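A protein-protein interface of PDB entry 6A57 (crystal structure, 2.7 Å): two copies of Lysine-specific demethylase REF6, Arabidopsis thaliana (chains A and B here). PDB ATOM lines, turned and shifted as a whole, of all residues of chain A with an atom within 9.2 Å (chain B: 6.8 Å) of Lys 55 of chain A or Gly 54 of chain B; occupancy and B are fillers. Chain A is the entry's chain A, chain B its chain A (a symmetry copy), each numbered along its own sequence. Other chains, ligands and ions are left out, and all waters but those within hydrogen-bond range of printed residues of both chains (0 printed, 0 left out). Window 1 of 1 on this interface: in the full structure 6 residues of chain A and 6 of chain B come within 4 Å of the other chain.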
ATOM      1  N   LEU A  42      28.547   5.552  -1.174  1.00  0.00           N
ATOM      2  CA  LEU A  42      28.312   6.908  -0.658  1.00  0.00           C
ATOM      3  C   LEU A  42      29.628   7.624  -0.344  1.00  0.00           C
ATOM      4  O   LEU A  42      29.823   8.772  -0.748  1.00  0.00           O
ATOM      5  CB  LEU A  42      27.429   6.871   0.598  1.00  0.00           C
ATOM      6  CG  LEU A  42      25.972   6.426   0.416  1.00  0.00           C
ATOM      7  CD1 LEU A  42      25.330   6.130   1.766  1.00  0.00           C
ATOM      8  CD2 LEU A  42      25.158   7.461  -0.349  1.00  0.00           C
ATOM      9  N   HIS A  43      30.519   6.942   0.374  1.00  0.00           N
ATOM     10  CA  HIS A  43      31.848   7.475   0.695  1.00  0.00           C
ATOM     11  C   HIS A  43      32.567   7.964  -0.553  1.00  0.00           C
ATOM     12  O   HIS A  43      33.100   9.074  -0.568  1.00  0.00           O
ATOM     13  CB  HIS A  43      32.703   6.413   1.394  1.00  0.00           C
ATOM     14  CG  HIS A  43      34.141   6.803   1.568  1.00  0.00           C
ATOM     15  ND1 HIS A  43      34.632   7.339   2.739  1.00  0.00           N
ATOM     16  CD2 HIS A  43      35.195   6.720   0.721  1.00  0.00           C
ATOM     17  CE1 HIS A  43      35.927   7.573   2.606  1.00  0.00           C
ATOM     18  NE2 HIS A  43      36.292   7.209   1.389  1.00  0.00           N
ATOM     19  N   ARG A  45      31.457   9.079  -3.334  1.00  0.00           N
ATOM     20  CA  ARG A  45      30.888  10.326  -3.880  1.00  0.00           C
ATOM     21  C   ARG A  45      30.758  11.480  -2.849  1.00  0.00           C
ATOM     22  O   ARG A  45      29.898  12.356  -2.997  1.00  0.00           O
ATOM     23  CB  ARG A  45      29.559  10.037  -4.602  1.00  0.00           C
ATOM     24  CG  ARG A  45      28.403   9.587  -3.721  1.00  0.00           C
ATOM     25  CD  ARG A  45      27.156   9.269  -4.534  1.00  0.00           C
ATOM     26  NE  ARG A  45      26.581  10.467  -5.157  1.00  0.00           N
ATOM     27  CZ  ARG A  45      25.333  10.575  -5.620  1.00  0.00           C
ATOM     28  NH1 ARG A  45      24.465   9.563  -5.535  1.00  0.00           N
ATOM     29  NH2 ARG A  45      24.941  11.724  -6.167  1.00  0.00           N
ATOM     30  N   ASN A  46      31.631  11.484  -1.834  1.00  0.00           N
ATOM     31  CA  ASN A  46      31.722  12.549  -0.811  1.00  0.00           C
ATOM     32  C   ASN A  46      30.455  12.729   0.039  1.00  0.00           C
ATOM     33  O   ASN A  46      29.969  13.850   0.225  1.00  0.00           O
ATOM     34  CB  ASN A  46      32.171  13.886  -1.436  1.00  0.00           C
ATOM     35  CG  ASN A  46      33.600  13.849  -1.957  1.00  0.00           C
ATOM     36  OD1 ASN A  46      34.273  12.814  -1.931  1.00  0.00           O
ATOM     37  ND2 ASN A  46      34.074  14.995  -2.427  1.00  0.00           N
ATOM     38  N   ILE A  47      29.934  11.613   0.549  1.00  0.00           N
ATOM     39  CA  ILE A  47      28.812  11.616   1.495  1.00  0.00           C
ATOM     40  C   ILE A  47      29.193  10.759   2.690  1.00  0.00           C
ATOM     41  O   ILE A  47      29.735   9.670   2.509  1.00  0.00           O
ATOM     42  CB  ILE A  47      27.511  11.061   0.879  1.00  0.00           C
ATOM     43  CG1 ILE A  47      27.154  11.819  -0.405  1.00  0.00           C
ATOM     44  CG2 ILE A  47      26.362  11.166   1.883  1.00  0.00           C
ATOM     45  CD1 ILE A  47      25.993  11.223  -1.181  1.00  0.00           C
ATOM     46  N   CYS A  48      28.905  11.240   3.901  1.00  0.00           N
ATOM     47  CA  CYS A  48      29.179  10.463   5.114  1.00  0.00           C
ATOM     48  C   CYS A  48      28.109   9.382   5.270  1.00  0.00           C
ATOM     49  O   CYS A  48      26.934   9.701   5.476  1.00  0.00           O
ATOM     50  CB  CYS A  48      29.217  11.338   6.366  1.00  0.00           C
ATOM     51  SG  CYS A  48      29.801  10.467   7.842  1.00  0.00           S
ATOM     52  N   PRO A  49      28.510   8.101   5.169  1.00  0.00           N
ATOM     53  CA  PRO A  49      27.533   7.019   5.227  1.00  0.00           C
ATOM     54  C   PRO A  49      26.973   6.735   6.625  1.00  0.00           C
ATOM     55  O   PRO A  49      25.896   6.141   6.719  1.00  0.00           O
ATOM     56  CB  PRO A  49      28.332   5.816   4.726  1.00  0.00           C
ATOM     57  CG  PRO A  49      29.719   6.090   5.201  1.00  0.00           C
ATOM     58  CD  PRO A  49      29.892   7.582   5.104  1.00  0.00           C
ATOM     59  N   ILE A  50      27.681   7.142   7.685  1.00  0.00           N
ATOM     60  CA  ILE A  50      27.237   6.907   9.071  1.00  0.00           C
ATOM     61  C   ILE A  50      25.753   7.250   9.206  1.00  0.00           C
ATOM     62  O   ILE A  50      25.300   8.262   8.674  1.00  0.00           O
ATOM     63  CB  ILE A  50      28.106   7.687  10.110  1.00  0.00           C
ATOM     64  CG1 ILE A  50      29.322   6.853  10.542  1.00  0.00           C
ATOM     65  CG2 ILE A  50      27.327   8.051  11.375  1.00  0.00           C
ATOM     66  CD1 ILE A  50      30.353   6.638   9.461  1.00  0.00           C
ATOM     67  N   LYS A  51      25.005   6.394   9.902  1.00  0.00           N
ATOM     68  CA  LYS A  51      23.552   6.553  10.001  1.00  0.00           C
ATOM     69  C   LYS A  51      23.235   7.816  10.804  1.00  0.00           C
ATOM     70  O   LYS A  51      23.853   8.064  11.834  1.00  0.00           O
ATOM     71  CB  LYS A  51      22.885   5.315  10.625  1.00  0.00           C
ATOM     72  CG  LYS A  51      21.459   5.096  10.127  1.00  0.00           C
ATOM     73  CD  LYS A  51      20.577   4.272  11.065  1.00  0.00           C
ATOM     74  CE  LYS A  51      20.888   2.779  11.015  1.00  0.00           C
ATOM     75  NZ  LYS A  51      20.516   2.119   9.730  1.00  0.00           N
ATOM     76  N   GLY A  52      22.307   8.629  10.299  1.00  0.00           N
ATOM     77  CA  GLY A  52      21.939   9.905  10.929  1.00  0.00           C
ATOM     78  C   GLY A  52      22.690  11.137  10.439  1.00  0.00           C
ATOM     79  O   GLY A  52      22.260  12.257  10.711  1.00  0.00           O
ATOM     80  N   CYS A  53      23.802  10.944   9.722  1.00  0.00           N
ATOM     81  CA  CYS A  53      24.610  12.051   9.201  1.00  0.00           C
ATOM     82  C   CYS A  53      24.186  12.388   7.762  1.00  0.00           C
ATOM     83  O   CYS A  53      23.301  13.231   7.566  1.00  0.00           O
ATOM     84  CB  CYS A  53      26.104  11.716   9.329  1.00  0.00           C
ATOM     85  SG  CYS A  53      27.207  13.013   8.747  1.00  0.00           S
ATOM     86  N   GLY A  54      24.773  11.718   6.770  1.00  0.00           N
ATOM     87  CA  GLY A  54      24.399  11.912   5.364  1.00  0.00           C
ATOM     88  C   GLY A  54      24.758  13.270   4.783  1.00  0.00           C
ATOM     89  O   GLY A  54      24.095  13.745   3.857  1.00  0.00           O
ATOM     90  N   LYS A  55      25.811  13.889   5.316  1.00  0.00           N
ATOM     91  CA  LYS A  55      26.237  15.209   4.872  1.00  0.00           C
ATOM     92  C   LYS A  55      27.065  15.091   3.603  1.00  0.00           C
ATOM     93  O   LYS A  55      27.869  14.173   3.482  1.00  0.00           O
ATOM     94  CB  LYS A  55      27.073  15.906   5.950  1.00  0.00           C
ATOM     95  CG  LYS A  55      26.274  16.402   7.147  1.00  0.00           C
ATOM     96  CD  LYS A  55      27.154  17.195   8.100  1.00  0.00           C
ATOM     97  CE  LYS A  55      26.340  17.924   9.151  1.00  0.00           C
ATOM     98  NZ  LYS A  55      27.111  19.039   9.765  1.00  0.00           N
ATOM     99  N   ASN A  56      26.855  16.027   2.673  1.00  0.00           N
ATOM    100  CA  ASN A  56      27.713  16.192   1.494  1.00  0.00           C
ATOM    101  C   ASN A  56      28.946  16.988   1.885  1.00  0.00           C
ATOM    102  O   ASN A  56      28.892  17.809   2.798  1.00  0.00           O
ATOM    103  CB  ASN A  56      26.979  16.935   0.379  1.00  0.00           C
ATOM    104  CG  ASN A  56      25.735  16.213  -0.077  1.00  0.00           C
ATOM    105  OD1 ASN A  56      25.801  15.077  -0.540  1.00  0.00           O
ATOM    106  ND2 ASN A  56      24.587  16.866   0.056  1.00  0.00           N
ATOM    107  N   PHE A  57      30.057  16.744   1.198  1.00  0.00           N
ATOM    108  CA  PHE A  57      31.309  17.462   1.458  1.00  0.00           C
ATOM    109  C   PHE A  57      31.977  17.881   0.157  1.00  0.00           C
ATOM    110  O   PHE A  57      31.840  17.204  -0.862  1.00  0.00           O
ATOM    111  CB  PHE A  57      32.255  16.600   2.301  1.00  0.00           C
ATOM    112  CG  PHE A  57      31.722  16.304   3.671  1.00  0.00           C
ATOM    113  CD1 PHE A  57      30.928  15.184   3.892  1.00  0.00           C
ATOM    114  CD2 PHE A  57      31.976  17.163   4.734  1.00  0.00           C
ATOM    115  CE1 PHE A  57      30.410  14.918   5.146  1.00  0.00           C
ATOM    116  CE2 PHE A  57      31.460  16.900   5.995  1.00  0.00           C
ATOM    117  CZ  PHE A  57      30.676  15.776   6.199  1.00  0.00           C
ATOM    118  N   PHE A  58      32.691  19.002   0.200  1.00  0.00           N
ATOM    119  CA  PHE A  58      33.391  19.529  -0.979  1.00  0.00           C
ATOM    120  C   PHE A  58      34.675  18.740  -1.275  1.00  0.00           C
ATOM    121  O   PHE A  58      34.947  18.429  -2.433  1.00  0.00           O
ATOM    122  CB  PHE A  58      33.685  21.034  -0.814  1.00  0.00           C
ATOM    123  CG  PHE A  58      32.539  21.943  -1.224  1.00  0.00           C
ATOM    124  CD1 PHE A  58      31.197  21.570  -1.046  1.00  0.00           C
ATOM    125  CD2 PHE A  58      32.804  23.199  -1.777  1.00  0.00           C
ATOM    126  CE1 PHE A  58      30.162  22.423  -1.423  1.00  0.00           C
ATOM    127  CE2 PHE A  58      31.769  24.054  -2.153  1.00  0.00           C
ATOM    128  CZ  PHE A  58      30.447  23.665  -1.975  1.00  0.00           C
ATOM    129  N   SER A  59      35.442  18.414  -0.232  1.00  0.00           N
ATOM    130  CA  SER A  59      36.700  17.666  -0.356  1.00  0.00           C
ATOM    131  C   SER A  59      36.554  16.243   0.183  1.00  0.00           C
ATOM    132  O   SER A  59      36.002  16.042   1.267  1.00  0.00           O
ATOM    133  CB  SER A  59      37.812  18.388   0.409  1.00  0.00           C
ATOM    134  OG  SER A  59      38.932  17.544   0.620  1.00  0.00           O
ATOM    135  N   TYR A  62      38.710  15.786   3.416  1.00  0.00           N
ATOM    136  CA  TYR A  62      38.012  16.214   4.640  1.00  0.00           C
ATOM    137  C   TYR A  62      37.037  15.145   5.162  1.00  0.00           C
ATOM    138  O   TYR A  62      36.889  15.004   6.378  1.00  0.00           O
ATOM    139  CB  TYR A  62      37.285  17.569   4.473  1.00  0.00           C
ATOM    140  CG  TYR A  62      36.652  18.024   5.774  1.00  0.00           C
ATOM    141  CD1 TYR A  62      37.442  18.455   6.841  1.00  0.00           C
ATOM    142  CD2 TYR A  62      35.274  17.955   5.963  1.00  0.00           C
ATOM    143  CE1 TYR A  62      36.873  18.836   8.051  1.00  0.00           C
ATOM    144  CE2 TYR A  62      34.693  18.334   7.166  1.00  0.00           C
ATOM    145  CZ  TYR A  62      35.492  18.774   8.210  1.00  0.00           C
ATOM    146  OH  TYR A  62      34.926  19.154   9.412  1.00  0.00           O
ATOM    147  N   LEU A  63      36.394  14.392   4.265  1.00  0.00           N
ATOM    148  CA  LEU A  63      35.491  13.287   4.665  1.00  0.00           C
ATOM    149  C   LEU A  63      36.119  12.351   5.710  1.00  0.00           C
ATOM    150  O   LEU A  63      35.434  11.874   6.602  1.00  0.00           O
ATOM    151  CB  LEU A  63      35.019  12.471   3.446  1.00  0.00           C
ATOM    152  CG  LEU A  63      33.535  12.079   3.410  1.00  0.00           C
ATOM    153  CD1 LEU A  63      33.265  11.151   2.233  1.00  0.00           C
ATOM    154  CD2 LEU A  63      33.050  11.428   4.702  1.00  0.00           C
ATOM    155  N   HIS A  66      36.422  14.635   8.852  1.00  0.00           N
ATOM    156  CA  HIS A  66      35.055  14.733   9.372  1.00  0.00           C
ATOM    157  C   HIS A  66      34.692  13.628  10.356  1.00  0.00           C
ATOM    158  O   HIS A  66      33.962  13.871  11.318  1.00  0.00           O
ATOM    159  CB  HIS A  66      34.042  14.716   8.216  1.00  0.00           C
ATOM    160  CG  HIS A  66      32.642  14.399   8.641  1.00  0.00           C
ATOM    161  ND1 HIS A  66      31.838  15.308   9.289  1.00  0.00           N
ATOM    162  CD2 HIS A  66      31.912  13.266   8.527  1.00  0.00           C
ATOM    163  CE1 HIS A  66      30.669  14.751   9.551  1.00  0.00           C
ATOM    164  NE2 HIS A  66      30.686  13.512   9.095  1.00  0.00           N
ATOM    165  N   GLN A  67      35.209  12.423  10.131  1.00  0.00           N
ATOM    166  CA  GLN A  67      34.831  11.261  10.943  1.00  0.00           C
ATOM    167  C   GLN A  67      35.071  11.424  12.445  1.00  0.00           C
ATOM    168  O   GLN A  67      34.468  10.694  13.236  1.00  0.00           O
ATOM    169  CB  GLN A  67      35.523   9.981  10.441  1.00  0.00           C
ATOM    170  CG  GLN A  67      35.146   9.536   9.029  1.00  0.00           C
ATOM    171  CD  GLN A  67      33.642   9.406   8.805  1.00  0.00           C
ATOM    172  OE1 GLN A  67      32.947   8.710   9.556  1.00  0.00           O
ATOM    173  NE2 GLN A  67      33.134  10.060   7.754  1.00  0.00           N
ATOM    174  N   VAL A  69      33.992  13.745  14.379  1.00  0.00           N
ATOM    175  CA  VAL A  69      32.742  14.142  15.053  1.00  0.00           C
ATOM    176  C   VAL A  69      31.948  12.928  15.520  1.00  0.00           C
ATOM    177  O   VAL A  69      31.184  13.013  16.481  1.00  0.00           O
ATOM    178  CB  VAL A  69      31.813  15.041  14.188  1.00  0.00           C
ATOM    179  CG1 VAL A  69      32.527  16.322  13.772  1.00  0.00           C
ATOM    180  CG2 VAL A  69      31.257  14.302  12.977  1.00  0.00           C
ATOM    181  N   HIS A  70      32.128  11.805  14.833  1.00  0.00           N
ATOM    182  CA  HIS A  70      31.477  10.561  15.213  1.00  0.00           C
ATOM    183  C   HIS A  70      32.246   9.796  16.303  1.00  0.00           C
ATOM    184  O   HIS A  70      31.636   9.069  17.078  1.00  0.00           O
ATOM    185  CB  HIS A  70      31.207   9.721  13.965  1.00  0.00           C
ATOM    186  CG  HIS A  70      30.372  10.440  12.946  1.00  0.00           C
ATOM    187  ND1 HIS A  70      29.084  10.856  13.203  1.00  0.00           N
ATOM    188  CD2 HIS A  70      30.652  10.851  11.685  1.00  0.00           C
ATOM    189  CE1 HIS A  70      28.604  11.482  12.144  1.00  0.00           C
ATOM    190  NE2 HIS A  70      29.533  11.485  11.206  1.00  0.00           N
ATOM    191  N   ILE B  47      18.705  18.541  -0.471  1.00  0.00           N
ATOM    192  CA  ILE B  47      19.877  18.880   0.344  1.00  0.00           C
ATOM    193  C   ILE B  47      19.554  20.125   1.151  1.00  0.00           C
ATOM    194  O   ILE B  47      18.992  21.073   0.607  1.00  0.00           O
ATOM    195  CB  ILE B  47      21.136  19.151  -0.506  1.00  0.00           C
ATOM    196  CG1 ILE B  47      21.431  17.964  -1.432  1.00  0.00           C
ATOM    197  CG2 ILE B  47      22.340  19.415   0.399  1.00  0.00           C
ATOM    198  CD1 ILE B  47      22.540  18.215  -2.437  1.00  0.00           C
ATOM    199  N   CYS B  48      19.913  20.127   2.436  1.00  0.00           N
ATOM    200  CA  CYS B  48      19.699  21.304   3.284  1.00  0.00           C
ATOM    201  C   CYS B  48      20.764  22.354   2.967  1.00  0.00           C
ATOM    202  O   CYS B  48      21.952  22.122   3.212  1.00  0.00           O
ATOM    203  CB  CYS B  48      19.739  20.960   4.772  1.00  0.00           C
ATOM    204  SG  CYS B  48      19.228  22.326   5.847  1.00  0.00           S
ATOM    205  N   PRO B  49      20.345  23.508   2.417  1.00  0.00           N
ATOM    206  CA  PRO B  49      21.311  24.523   2.013  1.00  0.00           C
ATOM    207  C   PRO B  49      21.945  25.303   3.171  1.00  0.00           C
ATOM    208  O   PRO B  49      23.018  25.878   2.976  1.00  0.00           O
ATOM    209  CB  PRO B  49      20.473  25.461   1.144  1.00  0.00           C
ATOM    210  CG  PRO B  49      19.118  25.399   1.763  1.00  0.00           C
ATOM    211  CD  PRO B  49      18.955  23.981   2.240  1.00  0.00           C
ATOM    212  N   ILE B  50      21.300  25.329   4.344  1.00  0.00           N
ATOM    213  CA  ILE B  50      21.818  26.059   5.515  1.00  0.00           C
ATOM    214  C   ILE B  50      23.311  25.776   5.686  1.00  0.00           C
ATOM    215  O   ILE B  50      23.744  24.633   5.546  1.00  0.00           O
ATOM    216  CB  ILE B  50      21.016  25.732   6.816  1.00  0.00           C
ATOM    217  CG1 ILE B  50      19.817  26.680   6.972  1.00  0.00           C
ATOM    218  CG2 ILE B  50      21.868  25.859   8.081  1.00  0.00           C
ATOM    219  CD1 ILE B  50      18.726  26.488   5.947  1.00  0.00           C
ATOM    220  N   LYS B  51      24.087  26.822   5.970  1.00  0.00           N
ATOM    221  CA  LYS B  51      25.545  26.695   6.040  1.00  0.00           C
ATOM    222  C   LYS B  51      25.919  25.820   7.238  1.00  0.00           C
ATOM    223  O   LYS B  51      25.362  25.981   8.319  1.00  0.00           O
ATOM    224  CB  LYS B  51      26.232  28.069   6.120  1.00  0.00           C
ATOM    225  CG  LYS B  51      27.626  28.071   5.498  1.00  0.00           C
ATOM    226  CD  LYS B  51      28.550  29.177   6.010  1.00  0.00           C
ATOM    227  CE  LYS B  51      28.220  30.546   5.424  1.00  0.00           C
ATOM    228  NZ  LYS B  51      28.514  30.674   3.967  1.00  0.00           N
ATOM    229  N   GLY B  52      26.826  24.868   7.023  1.00  0.00           N
ATOM    230  CA  GLY B  52      27.242  23.915   8.062  1.00  0.00           C
ATOM    231  C   GLY B  52      26.479  22.597   8.110  1.00  0.00           C
ATOM    232  O   GLY B  52      26.935  21.655   8.756  1.00  0.00           O
ATOM    233  N   CYS B  53      25.327  22.520   7.435  1.00  0.00           N
ATOM    234  CA  CYS B  53      24.503  21.308   7.410  1.00  0.00           C
ATOM    235  C   CYS B  53      24.851  20.453   6.180  1.00  0.00           C
ATOM    236  O   CYS B  53      25.732  19.589   6.264  1.00  0.00           O
ATOM    237  CB  CYS B  53      23.015  21.682   7.487  1.00  0.00           C
ATOM    238  SG  CYS B  53      21.896  20.273   7.492  1.00  0.00           S
ATOM    239  N   GLY B  54      24.203  20.711   5.043  1.00  0.00           N
ATOM    240  CA  GLY B  54      24.501  20.002   3.793  1.00  0.00           C
ATOM    241  C   GLY B  54      24.125  18.529   3.782  1.00  0.00           C
ATOM    242  O   GLY B  54      24.740  17.736   3.065  1.00  0.00           O
ATOM    243  N   LYS B  55      23.109  18.165   4.564  1.00  0.00           N
ATOM    244  CA  LYS B  55      22.673  16.780   4.670  1.00  0.00           C
ATOM    245  C   LYS B  55      21.776  16.424   3.496  1.00  0.00           C
ATOM    246  O   LYS B  55      20.956  17.240   3.086  1.00  0.00           O
ATOM    247  CB  LYS B  55      21.905  16.544   5.975  1.00  0.00           C
ATOM    248  CG  LYS B  55      22.775  16.522   7.224  1.00  0.00           C
ATOM    249  CD  LYS B  55      21.957  16.152   8.451  1.00  0.00           C
ATOM    250  CE  LYS B  55      22.835  15.860   9.651  1.00  0.00           C
ATOM    251  NZ  LYS B  55      22.112  15.063  10.678  1.00  0.00           N
ATOM    252  N   ASN B  56      21.944  15.206   2.973  1.00  0.00           N
ATOM    253  CA  ASN B  56      21.024  14.622   1.990  1.00  0.00           C
ATOM    254  C   ASN B  56      19.823  14.043   2.717  1.00  0.00           C
ATOM    255  O   ASN B  56      19.936  13.622   3.866  1.00  0.00           O
ATOM    256  CB  ASN B  56      21.703  13.510   1.194  1.00  0.00           C
ATOM    257  CG  ASN B  56      22.913  13.996   0.434  1.00  0.00           C
ATOM    258  OD1 ASN B  56      22.809  14.878  -0.416  1.00  0.00           O
ATOM    259  ND2 ASN B  56      24.073  13.427   0.737  1.00  0.00           N
ATOM    260  N   PHE B  57      18.673  14.025   2.052  1.00  0.00           N
ATOM    261  CA  PHE B  57      17.445  13.469   2.630  1.00  0.00           C
ATOM    262  C   PHE B  57      16.711  12.603   1.617  1.00  0.00           C
ATOM    263  O   PHE B  57      16.784  12.849   0.414  1.00  0.00           O
ATOM    264  CB  PHE B  57      16.538  14.594   3.141  1.00  0.00           C
ATOM    265  CG  PHE B  57      17.143  15.375   4.269  1.00  0.00           C
ATOM    266  CD1 PHE B  57      17.935  16.487   4.012  1.00  0.00           C
ATOM    267  CD2 PHE B  57      16.957  14.977   5.588  1.00  0.00           C
ATOM    268  CE1 PHE B  57      18.519  17.197   5.045  1.00  0.00           C
ATOM    269  CE2 PHE B  57      17.538  15.686   6.629  1.00  0.00           C
ATOM    270  CZ  PHE B  57      18.321  16.797   6.356  1.00  0.00           C
ATOM    271  N   HIS B  66      12.718  18.907   8.704  1.00  0.00           N
ATOM    272  CA  HIS B  66      14.113  18.995   9.146  1.00  0.00           C
ATOM    273  C   HIS B  66      14.518  20.384   9.625  1.00  0.00           C
ATOM    274  O   HIS B  66      15.302  20.509  10.566  1.00  0.00           O
ATOM    275  CB  HIS B  66      15.060  18.568   8.013  1.00  0.00           C
ATOM    276  CG  HIS B  66      16.478  19.006   8.212  1.00  0.00           C
ATOM    277  ND1 HIS B  66      17.327  18.396   9.107  1.00  0.00           N
ATOM    278  CD2 HIS B  66      17.188  20.007   7.643  1.00  0.00           C
ATOM    279  CE1 HIS B  66      18.502  18.998   9.077  1.00  0.00           C
ATOM    280  NE2 HIS B  66      18.447  19.977   8.192  1.00  0.00           N
ATOM    281  N   HIS B  70      17.305  23.719  12.949  1.00  0.00           N
ATOM    282  CA  HIS B  70      17.963  25.008  12.800  1.00  0.00           C
ATOM    283  C   HIS B  70      17.247  26.132  13.567  1.00  0.00           C
ATOM    284  O   HIS B  70      17.891  27.089  13.979  1.00  0.00           O
ATOM    285  CB  HIS B  70      18.154  25.318  11.316  1.00  0.00           C
ATOM    286  CG  HIS B  70      18.940  24.261  10.595  1.00  0.00           C
ATOM    287  ND1 HIS B  70      20.244  23.958  10.918  1.00  0.00           N
ATOM    288  CD2 HIS B  70      18.595  23.413   9.596  1.00  0.00           C
ATOM    289  CE1 HIS B  70      20.672  22.977  10.144  1.00  0.00           C
ATOM    290  NE2 HIS B  70      19.693  22.634   9.327  1.00  0.00           N
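The backbone NH (N) of Ile 47 of chain A sits at hydrogen-bond distance from the backbone carbonyl oxygen (O) of Leu 42 of chain A, at 3.1 Å. O of Cys 48 of chain A lies within hydrogen-bond range of N of Gly 54 of chain A (3.2 Å). The backbone NH (N) of Cys 48 of chain A sits at hydrogen-bond distance from the backbone carbonyl oxygen (O) of Lys 55 of chain A, 3.1 Å away. N of Cys 48 of chain B sits at hydrogen-bond distance from O of Lys 55 of chain B. N of Gly 54 of chain B lies within hydrogen-bond range of O of Cys 48 of chain B, 3.2 Å away.
Of the 23 printed residues of chain A, 6 touch a printed residue of chain B. Printed residues of chain A that touch a printed residue of chain B: Ile 47, Gly 52, Cys 53, Gly 54, Lys 55 and Asn 56. Hydrophobic or aromatic side chains of chain A that line the printed part of chain B: Ile 47. Of the 13 printed residues of chain B, 6 touch a printed residue of chain A. Hydrophobic or aromatic side chains of chain B within 4 Å of the printed part of chain A: Ile 47. Among the printed residues, 12 pairs touch across the chains.
Gly 52 of chain A touches Lys 55 of chain B, and with the chains exchanged Lys 55 of chain A touches Gly 52 of chain B. Cys 53 of chain A touches Lys 55 of chain B, and with the chains exchanged Lys 55 of chain A touches Cys 53 of chain B. Gly 54 of chain A touches Lys 55 of chain B, and with the chains exchanged Lys 55 of chain A touches Gly 54 of chain B. Asn 56 of chain A touches its own counterpart, Asn 56 of chain B. 13 positions are printed for both chains. Of the 12 pairs that touch across the chains among the printed residues, 12 have their exchanged pair printed and touching as well.
The side-chain amide nitrogen (ND2) of Asn 56 of chain B sits at hydrogen-bond distance from the side-chain amide oxygen (OD1) of Asn 56 of chain A (2.7 Å). The backbone carbonyl oxygen (O) of Gly 52 of chain B is in hydrogen-bond range of the side-chain amino group (NZ) of Lys 55 of chain A, at 2.8 Å. The backbone carbonyl oxygen (O) of Gly 52 of chain A lies within hydrogen-bond range of the side-chain amino group (NZ) of Lys 55 of chain B (2.8 Å). O of Gly 54 of chain A sits at hydrogen-bond distance from N of Asn 56 of chain B. The backbone NH (N) of Asn 56 of chain A is in hydrogen-bond range of the backbone carbonyl oxygen (O) of Gly 54 of chain B, at 2.7 Å.
ND2 of Asn 56 of chain B touches CG2 of Ile 47 of chain A (3.4 Å). Lys 55 of chain B touches Cys 53 of chain A (CD to O, 3.3 Å). Lys 55 of chain B touches Gly 54 of chain A. O of Cys 53 of chain B touches CD of Lys 55 of chain A, 3.3 Å away. Lys 55 of chain A touches Gly 54 of chain B. CG of Lys 55 of chain B touches CG of Lys 55 of chain A, at 3.5 Å. Ile 47 of chain B touches Asn 56 of chain A (CG2 to ND2, 3.4 Å).
Printed residues of chain B within 4 Å of Cys 53 of chain A: Lys 55 (3.3 Å). Lys 55 of chain A touches four residues of chain B. Phe 58 of chain A touches none of the printed residues of chain B. His 66 of chain A touches none of the printed residues of chain B. Cys 53 of chain B touches just one residue of chain A: Lys 55 (3.3 Å). Of chain A, only Lys 55 (3.4 Å) and Asn 56 (2.7 Å) come within 4 Å of Gly 54 of chain B. Of the printed residues of chain A, Lys 55 of chain B touches Gly 52, Cys 53, Gly 54 and Lys 55. Of the printed residues of chain A, Asn 56 of chain B touches Ile 47 (3.4 Å), Gly 54 (2.7 Å) and Asn 56 (2.7 Å). The nearest residue of chain B that does not touch Lys 55 of chain A is Asn 56 of chain B (4.5 Å). The nearest printed residue of chain A that does not touch Asn 56 of chain B is Lys 55 of chain A (4.5 Å).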
